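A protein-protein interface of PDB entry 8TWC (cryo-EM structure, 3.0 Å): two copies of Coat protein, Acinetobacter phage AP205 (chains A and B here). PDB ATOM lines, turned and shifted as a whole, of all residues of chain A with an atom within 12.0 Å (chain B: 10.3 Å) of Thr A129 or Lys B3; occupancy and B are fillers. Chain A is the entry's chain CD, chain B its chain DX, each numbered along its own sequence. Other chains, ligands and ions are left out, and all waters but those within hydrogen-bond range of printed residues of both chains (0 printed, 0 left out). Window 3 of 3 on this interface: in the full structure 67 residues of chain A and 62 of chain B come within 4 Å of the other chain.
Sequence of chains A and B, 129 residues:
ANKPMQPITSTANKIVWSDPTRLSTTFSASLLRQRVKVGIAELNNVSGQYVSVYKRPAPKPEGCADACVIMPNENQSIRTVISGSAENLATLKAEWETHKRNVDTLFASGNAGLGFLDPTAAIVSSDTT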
ATOM      1  N   ALA A  94     -16.110  39.680   5.282  1.00  0.00           N
ATOM      2  CA  ALA A  94     -17.445  39.110   5.114  1.00  0.00           C
ATOM      3  C   ALA A  94     -17.481  37.657   5.579  1.00  0.00           C
ATOM      4  O   ALA A  94     -18.442  37.225   6.232  1.00  0.00           O
ATOM      5  CB  ALA A  94     -17.886  39.221   3.655  1.00  0.00           C
ATOM      6  N   GLU A  95     -16.439  36.891   5.249  1.00  0.00           N
ATOM      7  CA  GLU A  95     -16.340  35.516   5.726  1.00  0.00           C
ATOM      8  C   GLU A  95     -16.283  35.466   7.246  1.00  0.00           C
ATOM      9  O   GLU A  95     -16.868  34.574   7.865  1.00  0.00           O
ATOM     10  CB  GLU A  95     -15.108  34.836   5.129  1.00  0.00           C
ATOM     11  CG  GLU A  95     -15.173  34.585   3.633  1.00  0.00           C
ATOM     12  CD  GLU A  95     -16.361  33.737   3.229  1.00  0.00           C
ATOM     13  OE1 GLU A  95     -16.653  32.746   3.931  1.00  0.00           O
ATOM     14  OE2 GLU A  95     -16.992  34.053   2.200  1.00  0.00           O
ATOM     15  N   GLU A  97     -17.613  37.645   9.341  1.00  0.00           N
ATOM     16  CA  GLU A  97     -18.957  37.921   9.841  1.00  0.00           C
ATOM     17  C   GLU A  97     -19.856  36.696   9.715  1.00  0.00           C
ATOM     18  O   GLU A  97     -20.593  36.354  10.652  1.00  0.00           O
ATOM     19  CB  GLU A  97     -19.564  39.109   9.096  1.00  0.00           C
ATOM     20  CG  GLU A  97     -18.858  40.429   9.357  1.00  0.00           C
ATOM     21  CD  GLU A  97     -18.809  40.782  10.830  1.00  0.00           C
ATOM     22  OE1 GLU A  97     -19.858  40.689  11.501  1.00  0.00           O
ATOM     23  OE2 GLU A  97     -17.721  41.154  11.317  1.00  0.00           O
ATOM     24  N   THR A  98     -19.803  36.015   8.568  1.00  0.00           N
ATOM     25  CA  THR A  98     -20.618  34.818   8.385  1.00  0.00           C
ATOM     26  C   THR A  98     -20.206  33.713   9.353  1.00  0.00           C
ATOM     27  O   THR A  98     -21.059  32.993   9.886  1.00  0.00           O
ATOM     28  CB  THR A  98     -20.518  34.334   6.939  1.00  0.00           C
ATOM     29  OG1 THR A  98     -20.922  35.388   6.058  1.00  0.00           O
ATOM     30  CG2 THR A  98     -21.414  33.126   6.716  1.00  0.00           C
ATOM     31  N   HIS A  99     -18.902  33.563   9.585  1.00  0.00           N
ATOM     32  CA  HIS A  99     -18.415  32.567  10.531  1.00  0.00           C
ATOM     33  C   HIS A  99     -18.902  32.871  11.939  1.00  0.00           C
ATOM     34  O   HIS A  99     -19.303  31.967  12.680  1.00  0.00           O
ATOM     35  CB  HIS A  99     -16.889  32.514  10.484  1.00  0.00           C
ATOM     36  CG  HIS A  99     -16.288  31.497  11.399  1.00  0.00           C
ATOM     37  ND1 HIS A  99     -16.102  30.182  11.030  1.00  0.00           N
ATOM     38  CD2 HIS A  99     -15.826  31.600  12.667  1.00  0.00           C
ATOM     39  CE1 HIS A  99     -15.554  29.519  12.032  1.00  0.00           C
ATOM     40  NE2 HIS A  99     -15.377  30.357  13.038  1.00  0.00           N
ATOM     41  N   ARG A 101     -21.638  34.484  12.687  1.00  0.00           N
ATOM     42  CA  ARG A 101     -23.066  34.178  12.706  1.00  0.00           C
ATOM     43  C   ARG A 101     -23.315  32.681  12.862  1.00  0.00           C
ATOM     44  O   ARG A 101     -24.170  32.262  13.653  1.00  0.00           O
ATOM     45  CB  ARG A 101     -23.725  34.703  11.431  1.00  0.00           C
ATOM     46  CG  ARG A 101     -25.230  34.530  11.382  1.00  0.00           C
ATOM     47  CD  ARG A 101     -25.794  35.115  10.099  1.00  0.00           C
ATOM     48  NE  ARG A 101     -27.235  34.927  10.000  1.00  0.00           N
ATOM     49  CZ  ARG A 101     -27.976  35.351   8.985  1.00  0.00           C
ATOM     50  NH1 ARG A 101     -27.441  35.995   7.961  1.00  0.00           N
ATOM     51  NH2 ARG A 101     -29.287  35.124   8.999  1.00  0.00           N
ATOM     52  N   ASN A 102     -22.571  31.859  12.120  1.00  0.00           N
ATOM     53  CA  ASN A 102     -22.778  30.415  12.185  1.00  0.00           C
ATOM     54  C   ASN A 102     -22.372  29.853  13.544  1.00  0.00           C
ATOM     55  O   ASN A 102     -23.065  28.988  14.102  1.00  0.00           O
ATOM     56  CB  ASN A 102     -22.004  29.727  11.064  1.00  0.00           C
ATOM     57  CG  ASN A 102     -22.635  29.944   9.706  1.00  0.00           C
ATOM     58  OD1 ASN A 102     -23.854  30.064   9.588  1.00  0.00           O
ATOM     59  ND2 ASN A 102     -21.808  29.996   8.670  1.00  0.00           N
ATOM     60  N   THR A 105     -25.067  30.614  15.908  1.00  0.00           N
ATOM     61  CA  THR A 105     -26.207  29.721  15.737  1.00  0.00           C
ATOM     62  C   THR A 105     -25.962  28.377  16.412  1.00  0.00           C
ATOM     63  O   THR A 105     -26.854  27.835  17.074  1.00  0.00           O
ATOM     64  CB  THR A 105     -26.502  29.525  14.249  1.00  0.00           C
ATOM     65  OG1 THR A 105     -26.799  30.793  13.650  1.00  0.00           O
ATOM     66  CG2 THR A 105     -27.689  28.596  14.060  1.00  0.00           C
ATOM     67  N   ALA A 121     -30.026  22.969  12.354  1.00  0.00           N
ATOM     68  CA  ALA A 121     -29.656  24.359  12.580  1.00  0.00           C
ATOM     69  C   ALA A 121     -29.570  25.114  11.260  1.00  0.00           C
ATOM     70  O   ALA A 121     -29.181  24.558  10.230  1.00  0.00           O
ATOM     71  CB  ALA A 121     -28.322  24.437  13.321  1.00  0.00           C
ATOM     72  N   ALA A 122     -29.935  26.396  11.298  1.00  0.00           N
ATOM     73  CA  ALA A 122     -29.978  27.232  10.099  1.00  0.00           C
ATOM     74  C   ALA A 122     -28.610  27.873   9.890  1.00  0.00           C
ATOM     75  O   ALA A 122     -28.293  28.945  10.410  1.00  0.00           O
ATOM     76  CB  ALA A 122     -31.077  28.280  10.215  1.00  0.00           C
ATOM     77  N   ILE A 123     -27.783  27.192   9.102  1.00  0.00           N
ATOM     78  CA  ILE A 123     -26.443  27.654   8.763  1.00  0.00           C
ATOM     79  C   ILE A 123     -26.486  28.309   7.391  1.00  0.00           C
ATOM     80  O   ILE A 123     -27.076  27.764   6.449  1.00  0.00           O
ATOM     81  CB  ILE A 123     -25.435  26.489   8.795  1.00  0.00           C
ATOM     82  CG1 ILE A 123     -25.416  25.844  10.181  1.00  0.00           C
ATOM     83  CG2 ILE A 123     -24.049  26.979   8.449  1.00  0.00           C
ATOM     84  CD1 ILE A 123     -25.107  26.808  11.302  1.00  0.00           C
ATOM     85  N   VAL A 124     -25.861  29.481   7.269  1.00  0.00           N
ATOM     86  CA  VAL A 124     -25.925  30.279   6.051  1.00  0.00           C
ATOM     87  C   VAL A 124     -24.516  30.594   5.566  1.00  0.00           C
ATOM     88  O   VAL A 124     -23.550  30.556   6.333  1.00  0.00           O
ATOM     89  CB  VAL A 124     -26.721  31.587   6.262  1.00  0.00           C
ATOM     90  CG1 VAL A 124     -28.163  31.279   6.636  1.00  0.00           C
ATOM     91  CG2 VAL A 124     -26.060  32.445   7.328  1.00  0.00           C
ATOM     92  N   SER A 125     -24.408  30.902   4.276  1.00  0.00           N
ATOM     93  CA  SER A 125     -23.137  31.249   3.660  1.00  0.00           C
ATOM     94  C   SER A 125     -22.966  32.762   3.577  1.00  0.00           C
ATOM     95  O   SER A 125     -23.876  33.539   3.879  1.00  0.00           O
ATOM     96  CB  SER A 125     -23.030  30.654   2.257  1.00  0.00           C
ATOM     97  OG  SER A 125     -21.923  31.197   1.560  1.00  0.00           O
ATOM     98  N   SER A 126     -21.769  33.175   3.155  1.00  0.00           N
ATOM     99  CA  SER A 126     -21.492  34.594   2.974  1.00  0.00           C
ATOM    100  C   SER A 126     -22.151  35.159   1.726  1.00  0.00           C
ATOM    101  O   SER A 126     -22.452  36.356   1.687  1.00  0.00           O
ATOM    102  CB  SER A 126     -19.984  34.830   2.915  1.00  0.00           C
ATOM    103  OG  SER A 126     -19.420  34.224   1.766  1.00  0.00           O
ATOM    104  N   ASP A 127     -22.379  34.333   0.709  1.00  0.00           N
ATOM    105  CA  ASP A 127     -23.003  34.805  -0.516  1.00  0.00           C
ATOM    106  C   ASP A 127     -24.469  35.150  -0.273  1.00  0.00           C
ATOM    107  O   ASP A 127     -25.137  34.564   0.583  1.00  0.00           O
ATOM    108  CB  ASP A 127     -22.890  33.748  -1.613  1.00  0.00           C
ATOM    109  CG  ASP A 127     -21.485  33.635  -2.168  1.00  0.00           C
ATOM    110  OD1 ASP A 127     -20.755  34.649  -2.155  1.00  0.00           O
ATOM    111  OD2 ASP A 127     -21.108  32.532  -2.616  1.00  0.00           O
ATOM    112  N   THR A 128     -24.966  36.114  -1.039  1.00  0.00           N
ATOM    113  CA  THR A 128     -26.340  36.574  -0.934  1.00  0.00           C
ATOM    114  C   THR A 128     -27.108  36.242  -2.206  1.00  0.00           C
ATOM    115  O   THR A 128     -26.526  36.026  -3.273  1.00  0.00           O
ATOM    116  CB  THR A 128     -26.399  38.083  -0.671  1.00  0.00           C
ATOM    117  OG1 THR A 128     -26.081  38.791  -1.875  1.00  0.00           O
ATOM    118  CG2 THR A 128     -25.412  38.474   0.418  1.00  0.00           C
ATOM    119  N   THR A 129     -28.429  36.202  -2.079  1.00  0.00           N
ATOM    120  CA  THR A 129     -29.297  35.895  -3.208  1.00  0.00           C
ATOM    121  C   THR A 129     -29.621  37.153  -4.006  1.00  0.00           C
ATOM    122  O   THR A 129     -30.456  37.129  -4.909  1.00  0.00           O
ATOM    123  CB  THR A 129     -30.610  35.239  -2.749  1.00  0.00           C
ATOM    124  OG1 THR A 129     -31.338  36.153  -1.919  1.00  0.00           O
ATOM    125  CG2 THR A 129     -30.322  33.969  -1.964  1.00  0.00           C
ATOM    126  N   ALA B   1     -30.433  38.296   2.061  1.00  0.00           N
ATOM    127  CA  ALA B   1     -30.780  36.889   2.221  1.00  0.00           C
ATOM    128  C   ALA B   1     -29.597  35.995   1.878  1.00  0.00           C
ATOM    129  O   ALA B   1     -29.300  35.762   0.706  1.00  0.00           O
ATOM    130  CB  ALA B   1     -31.980  36.537   1.356  1.00  0.00           C
ATOM    131  N   ASN B   2     -28.920  35.497   2.909  1.00  0.00           N
ATOM    132  CA  ASN B   2     -27.769  34.631   2.699  1.00  0.00           C
ATOM    133  C   ASN B   2     -28.215  33.257   2.211  1.00  0.00           C
ATOM    134  O   ASN B   2     -29.288  32.769   2.574  1.00  0.00           O
ATOM    135  CB  ASN B   2     -26.968  34.500   3.992  1.00  0.00           C
ATOM    136  CG  ASN B   2     -26.219  35.767   4.342  1.00  0.00           C
ATOM    137  OD1 ASN B   2     -26.795  36.712   4.880  1.00  0.00           O
ATOM    138  ND2 ASN B   2     -24.927  35.796   4.039  1.00  0.00           N
ATOM    139  N   LYS B   3     -27.384  32.637   1.386  1.00  0.00           N
ATOM    140  CA  LYS B   3     -27.709  31.320   0.855  1.00  0.00           C
ATOM    141  C   LYS B   3     -27.555  30.266   1.946  1.00  0.00           C
ATOM    142  O   LYS B   3     -26.484  30.165   2.556  1.00  0.00           O
ATOM    143  CB  LYS B   3     -26.808  30.985  -0.331  1.00  0.00           C
ATOM    144  CG  LYS B   3     -27.068  31.826  -1.567  1.00  0.00           C
ATOM    145  CD  LYS B   3     -26.098  31.478  -2.683  1.00  0.00           C
ATOM    146  CE  LYS B   3     -26.733  31.689  -4.047  1.00  0.00           C
ATOM    147  NZ  LYS B   3     -25.785  31.381  -5.155  1.00  0.00           N
ATOM    148  N   PRO B   4     -28.584  29.470   2.221  1.00  0.00           N
ATOM    149  CA  PRO B   4     -28.465  28.448   3.263  1.00  0.00           C
ATOM    150  C   PRO B   4     -27.701  27.229   2.775  1.00  0.00           C
ATOM    151  O   PRO B   4     -27.550  27.000   1.573  1.00  0.00           O
ATOM    152  CB  PRO B   4     -29.922  28.100   3.578  1.00  0.00           C
ATOM    153  CG  PRO B   4     -30.631  28.351   2.292  1.00  0.00           C
ATOM    154  CD  PRO B   4     -29.948  29.540   1.668  1.00  0.00           C
ATOM    155  N   MET B   5     -27.215  26.440   3.731  1.00  0.00           N
ATOM    156  CA  MET B   5     -26.500  25.208   3.443  1.00  0.00           C
ATOM    157  C   MET B   5     -27.259  24.015   4.007  1.00  0.00           C
ATOM    158  O   MET B   5     -28.163  24.164   4.834  1.00  0.00           O
ATOM    159  CB  MET B   5     -25.078  25.228   4.014  1.00  0.00           C
ATOM    160  CG  MET B   5     -24.095  26.022   3.178  1.00  0.00           C
ATOM    161  SD  MET B   5     -23.883  27.712   3.745  1.00  0.00           S
ATOM    162  CE  MET B   5     -22.805  27.470   5.150  1.00  0.00           C
ATOM    163  N   GLN B   6     -26.880  22.825   3.541  1.00  0.00           N
ATOM    164  CA  GLN B   6     -27.447  21.564   3.977  1.00  0.00           C
ATOM    165  C   GLN B   6     -26.338  20.602   4.382  1.00  0.00           C
ATOM    166  O   GLN B   6     -25.237  20.661   3.824  1.00  0.00           O
ATOM    167  CB  GLN B   6     -28.286  20.928   2.862  1.00  0.00           C
ATOM    168  CG  GLN B   6     -29.466  21.772   2.420  1.00  0.00           C
ATOM    169  CD  GLN B   6     -30.512  21.928   3.505  1.00  0.00           C
ATOM    170  OE1 GLN B   6     -30.804  20.986   4.241  1.00  0.00           O
ATOM    171  NE2 GLN B   6     -31.080  23.124   3.612  1.00  0.00           N
ATOM    172  N   TRP B  17     -21.346  21.232   6.544  1.00  0.00           N
ATOM    173  CA  TRP B  17     -22.369  21.838   5.707  1.00  0.00           C
ATOM    174  C   TRP B  17     -21.754  22.293   4.390  1.00  0.00           C
ATOM    175  O   TRP B  17     -20.580  22.661   4.329  1.00  0.00           O
ATOM    176  CB  TRP B  17     -23.018  23.028   6.413  1.00  0.00           C
ATOM    177  CG  TRP B  17     -23.970  22.649   7.502  1.00  0.00           C
ATOM    178  CD1 TRP B  17     -25.326  22.553   7.408  1.00  0.00           C
ATOM    179  CD2 TRP B  17     -23.637  22.318   8.853  1.00  0.00           C
ATOM    180  NE1 TRP B  17     -25.858  22.182   8.618  1.00  0.00           N
ATOM    181  CE2 TRP B  17     -24.841  22.031   9.522  1.00  0.00           C
ATOM    182  CE3 TRP B  17     -22.436  22.235   9.563  1.00  0.00           C
ATOM    183  CZ2 TRP B  17     -24.880  21.667  10.863  1.00  0.00           C
ATOM    184  CZ3 TRP B  17     -22.478  21.874  10.895  1.00  0.00           C
ATOM    185  CH2 TRP B  17     -23.691  21.595  11.531  1.00  0.00           C
ATOM    186  N   SER B  18     -22.558  22.263   3.329  1.00  0.00           N
ATOM    187  CA  SER B  18     -22.077  22.653   2.013  1.00  0.00           C
ATOM    188  C   SER B  18     -23.196  23.335   1.243  1.00  0.00           C
ATOM    189  O   SER B  18     -24.368  22.970   1.362  1.00  0.00           O
ATOM    190  CB  SER B  18     -21.554  21.449   1.223  1.00  0.00           C
ATOM    191  OG  SER B  18     -22.443  20.350   1.323  1.00  0.00           O
ATOM    192  N   ASP B  19     -22.817  24.331   0.451  1.00  0.00           N
ATOM    193  CA  ASP B  19     -23.772  25.054  -0.377  1.00  0.00           C
ATOM    194  C   ASP B  19     -24.083  24.236  -1.623  1.00  0.00           C
ATOM    195  O   ASP B  19     -23.156  23.846  -2.342  1.00  0.00           O
ATOM    196  CB  ASP B  19     -23.209  26.416  -0.764  1.00  0.00           C
ATOM    197  CG  ASP B  19     -24.232  27.311  -1.442  1.00  0.00           C
ATOM    198  OD1 ASP B  19     -25.369  26.860  -1.692  1.00  0.00           O
ATOM    199  OD2 ASP B  19     -23.893  28.478  -1.731  1.00  0.00           O
ATOM    200  N   PRO B  20     -25.353  23.938  -1.906  1.00  0.00           N
ATOM    201  CA  PRO B  20     -25.675  23.185  -3.129  1.00  0.00           C
ATOM    202  C   PRO B  20     -25.181  23.847  -4.404  1.00  0.00           C
ATOM    203  O   PRO B  20     -24.846  23.137  -5.359  1.00  0.00           O
ATOM    204  CB  PRO B  20     -27.210  23.102  -3.110  1.00  0.00           C
ATOM    205  CG  PRO B  20     -27.660  23.738  -1.824  1.00  0.00           C
ATOM    206  CD  PRO B  20     -26.474  23.961  -0.956  1.00  0.00           C
ATOM    207  N   THR B  21     -25.127  25.175  -4.452  1.00  0.00           N
ATOM    208  CA  THR B  21     -24.666  25.879  -5.641  1.00  0.00           C
ATOM    209  C   THR B  21     -23.152  26.034  -5.696  1.00  0.00           C
ATOM    210  O   THR B  21     -22.599  26.161  -6.794  1.00  0.00           O
ATOM    211  CB  THR B  21     -25.315  27.263  -5.722  1.00  0.00           C
ATOM    212  OG1 THR B  21     -24.616  28.172  -4.863  1.00  0.00           O
ATOM    213  CG2 THR B  21     -26.772  27.192  -5.295  1.00  0.00           C
ATOM    214  N   ARG B  22     -22.471  26.028  -4.550  1.00  0.00           N
ATOM    215  CA  ARG B  22     -21.012  26.124  -4.517  1.00  0.00           C
ATOM    216  C   ARG B  22     -20.517  25.087  -3.512  1.00  0.00           C
ATOM    217  O   ARG B  22     -20.466  25.362  -2.310  1.00  0.00           O
ATOM    218  CB  ARG B  22     -20.553  27.526  -4.143  1.00  0.00           C
ATOM    219  CG  ARG B  22     -21.107  28.633  -5.024  1.00  0.00           C
ATOM    220  CD  ARG B  22     -20.449  28.634  -6.394  1.00  0.00           C
ATOM    221  NE  ARG B  22     -20.916  29.741  -7.220  1.00  0.00           N
ATOM    222  CZ  ARG B  22     -20.681  29.857  -8.520  1.00  0.00           C
ATOM    223  NH1 ARG B  22     -19.982  28.949  -9.180  1.00  0.00           N
ATOM    224  NH2 ARG B  22     -21.160  30.912  -9.174  1.00  0.00           N
ATOM    225  N   LEU B  23     -20.155  23.904  -4.012  1.00  0.00           N
ATOM    226  CA  LEU B  23     -19.714  22.831  -3.130  1.00  0.00           C
ATOM    227  C   LEU B  23     -18.364  23.121  -2.488  1.00  0.00           C
ATOM    228  O   LEU B  23     -17.994  22.442  -1.524  1.00  0.00           O
ATOM    229  CB  LEU B  23     -19.651  21.511  -3.898  1.00  0.00           C
ATOM    230  CG  LEU B  23     -20.983  20.964  -4.410  1.00  0.00           C
ATOM    231  CD1 LEU B  23     -20.785  19.616  -5.080  1.00  0.00           C
ATOM    232  CD2 LEU B  23     -21.985  20.857  -3.275  1.00  0.00           C
ATOM    233  N   THR B  25     -17.685  25.711  -0.766  1.00  0.00           N
ATOM    234  CA  THR B  25     -17.952  26.392   0.494  1.00  0.00           C
ATOM    235  C   THR B  25     -18.406  25.363   1.519  1.00  0.00           C
ATOM    236  O   THR B  25     -19.420  24.685   1.317  1.00  0.00           O
ATOM    237  CB  THR B  25     -19.015  27.475   0.319  1.00  0.00           C
ATOM    238  OG1 THR B  25     -18.680  28.298  -0.805  1.00  0.00           O
ATOM    239  CG2 THR B  25     -19.102  28.339   1.566  1.00  0.00           C
ATOM    240  N   THR B  26     -17.660  25.247   2.613  1.00  0.00           N
ATOM    241  CA  THR B  26     -17.937  24.259   3.645  1.00  0.00           C
ATOM    242  C   THR B  26     -17.877  24.911   5.017  1.00  0.00           C
ATOM    243  O   THR B  26     -17.170  25.900   5.225  1.00  0.00           O
ATOM    244  CB  THR B  26     -16.942  23.088   3.596  1.00  0.00           C
ATOM    245  OG1 THR B  26     -15.613  23.577   3.815  1.00  0.00           O
ATOM    246  CG2 THR B  26     -17.004  22.380   2.251  1.00  0.00           C
ATOM    247  N   PHE B  27     -18.632  24.342   5.954  1.00  0.00           N
ATOM    248  CA  PHE B  27     -18.594  24.747   7.354  1.00  0.00           C
ATOM    249  C   PHE B  27     -18.655  23.491   8.208  1.00  0.00           C
ATOM    250  O   PHE B  27     -19.606  22.710   8.097  1.00  0.00           O
ATOM    251  CB  PHE B  27     -19.745  25.693   7.694  1.00  0.00           C
ATOM    252  CG  PHE B  27     -19.705  26.208   9.101  1.00  0.00           C
ATOM    253  CD1 PHE B  27     -18.841  27.231   9.450  1.00  0.00           C
ATOM    254  CD2 PHE B  27     -20.525  25.673  10.074  1.00  0.00           C
ATOM    255  CE1 PHE B  27     -18.798  27.709  10.743  1.00  0.00           C
ATOM    256  CE2 PHE B  27     -20.486  26.148  11.367  1.00  0.00           C
ATOM    257  CZ  PHE B  27     -19.622  27.165  11.702  1.00  0.00           C
ATOM    258  N   TYR B  54     -13.840  28.912   2.240  1.00  0.00           N
ATOM    259  CA  TYR B  54     -14.367  29.519   1.028  1.00  0.00           C
ATOM    260  C   TYR B  54     -13.220  29.734   0.055  1.00  0.00           C
ATOM    261  O   TYR B  54     -12.183  30.294   0.422  1.00  0.00           O
ATOM    262  CB  TYR B  54     -15.063  30.850   1.325  1.00  0.00           C
ATOM    263  CG  TYR B  54     -15.945  31.353   0.204  1.00  0.00           C
ATOM    264  CD1 TYR B  54     -15.406  32.033  -0.877  1.00  0.00           C
ATOM    265  CD2 TYR B  54     -17.317  31.152   0.232  1.00  0.00           C
ATOM    266  CE1 TYR B  54     -16.207  32.496  -1.900  1.00  0.00           C
ATOM    267  CE2 TYR B  54     -18.126  31.611  -0.788  1.00  0.00           C
ATOM    268  CZ  TYR B  54     -17.566  32.282  -1.851  1.00  0.00           C
ATOM    269  OH  TYR B  54     -18.369  32.741  -2.869  1.00  0.00           O
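No position is printed for both chains.
The guanidinium group (NH1) of Arg A101 is in hydrogen-bond range of the side-chain amide oxygen (OD1) of Asn B2 (3.2 Å).
O of Ile A123 is in hydrogen-bond range of N of Met B5.
The backbone carbonyl oxygen of Ser A125 sits at hydrogen-bond distance from the side-chain amide nitrogen of Asn B2 (2.5 Å).
N of Ser A125 is in hydrogen-bond range of O of Lys B3.
The backbone NH (N) of Ser A125 lies within hydrogen-bond range of the side-chain sulfur (SD) of Met B5, 3.3 Å away.
ND2 of Asn B2 is in hydrogen-bond range of O of Ser A126.
N of Lys B3 is in hydrogen-bond range of O of Asp A127, 3.1 Å away.
OH of Tyr B54 lies within hydrogen-bond range of OD2 of Asp A127 (2.8 Å).
N of Thr A129 lies within hydrogen-bond range of O of Ala B1 (3.0 Å).
Of the 17 printed residues of chain B, 8 touch a printed residue of chain A.
Printed residues of chain B that touch a printed residue of chain A: Ala B1, Asn B2, Lys B3, Pro B4, Met B5, Trp B17, Phe B27 and Tyr B54.
Hydrophobic or aromatic side chains of chain B that line the printed part of chain A: Ala B1, Met B5, Trp B17, Phe B27 and Tyr B54.
Of the 17 printed residues of chain A, 11 touch a printed residue of chain B.
Hydrophobic or aromatic side chains of chain A within 4 Å of the printed part of chain B: His A99, Ile A123 and Val A124.
Among the printed residues, no Asp or Glu carboxylate lies within 4 Å of a Lys or Arg side-chain nitrogen of the other chain.
Of chain B, only Ala B1 and Lys B3 come within 4 Å of Thr A129.
Of chain A, only Val A124, Ser A125, Asp A127 and Thr A129 come within 4 Å of Lys B3.
Val A124 touches three residues of chain B.
Of chain B, only Asn B2, Lys B3 and Tyr B54 come within 4 Å of Asp A127.
Of chain A, only Arg A101 (3.2 Å), Val A124 (3.7 Å), Ser A125 (2.5 Å), Ser A126 (3.5 Å) and Asp A127 (3.4 Å) come within 4 Å of Asn B2.
Met B5 touches just these residues of chain A: Ile A123, Val A124 and Ser A125.
No residue of chain A comes within 4 Å of Thr B21.
Of the printed residues of chain A, Trp B17 touches Ile A123 (3.9 Å).
Of the printed residues of chain B, Ser A126 touches Asn B2 and Tyr B54.
Printed residues of chain A within 4 Å of Tyr B54: Glu A95 (3.5 Å), Ser A126 (3.9 Å) and Asp A127 (2.8 Å).
Printed residues of chain B within 4 Å of Ile A123: Pro B4, Met B5 and Trp B17.
Printed residues of chain B within 4 Å of His A99: Phe B27 (3.7 Å).
The nearest residue of chain A that does not touch Lys B3 is Thr A128 (4.4 Å).
Tyr B54 touches Glu A95.
His A99 touches Phe B27.
Phe B27 touches Asn A102.
O of Ile A123 touches CA of Pro B4, 3.5 Å away.
Ile A123 touches Trp B17 (CG1 to CE2, 3.9 Å).
Val A124 touches Met B5.
Ser A126 touches Tyr B54 (OG to CE2, 3.9 Å).
Asp A127 touches Asn B2 (O to CA, 3.4 Å).
Thr A128 touches Ala B1.
CG of Lys B3 touches CG2 of Thr A129 (3.9 Å).
The side-chain carboxylate (OE2) of Glu A95 is in hydrogen-bond range of the side-chain hydroxyl (OG) of Ser A126.
O of Thr A98 sits at hydrogen-bond distance from ND2 of Asn A102 (3.3 Å).
The side-chain hydroxyl of Thr A105 lies within hydrogen-bond range of the backbone carbonyl oxygen of Arg A101 (3.0 Å).
OG of Ser A125 lies within hydrogen-bond range of N of Asp A127, at 3.3 Å.
The side-chain amino group (NZ) of Lys B3 lies within hydrogen-bond range of the side-chain hydroxyl (OG1) of Thr B21 (3.4 Å).
The backbone NH of Trp B17 is in hydrogen-bond range of the backbone carbonyl oxygen of Phe B27 (2.8 Å).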
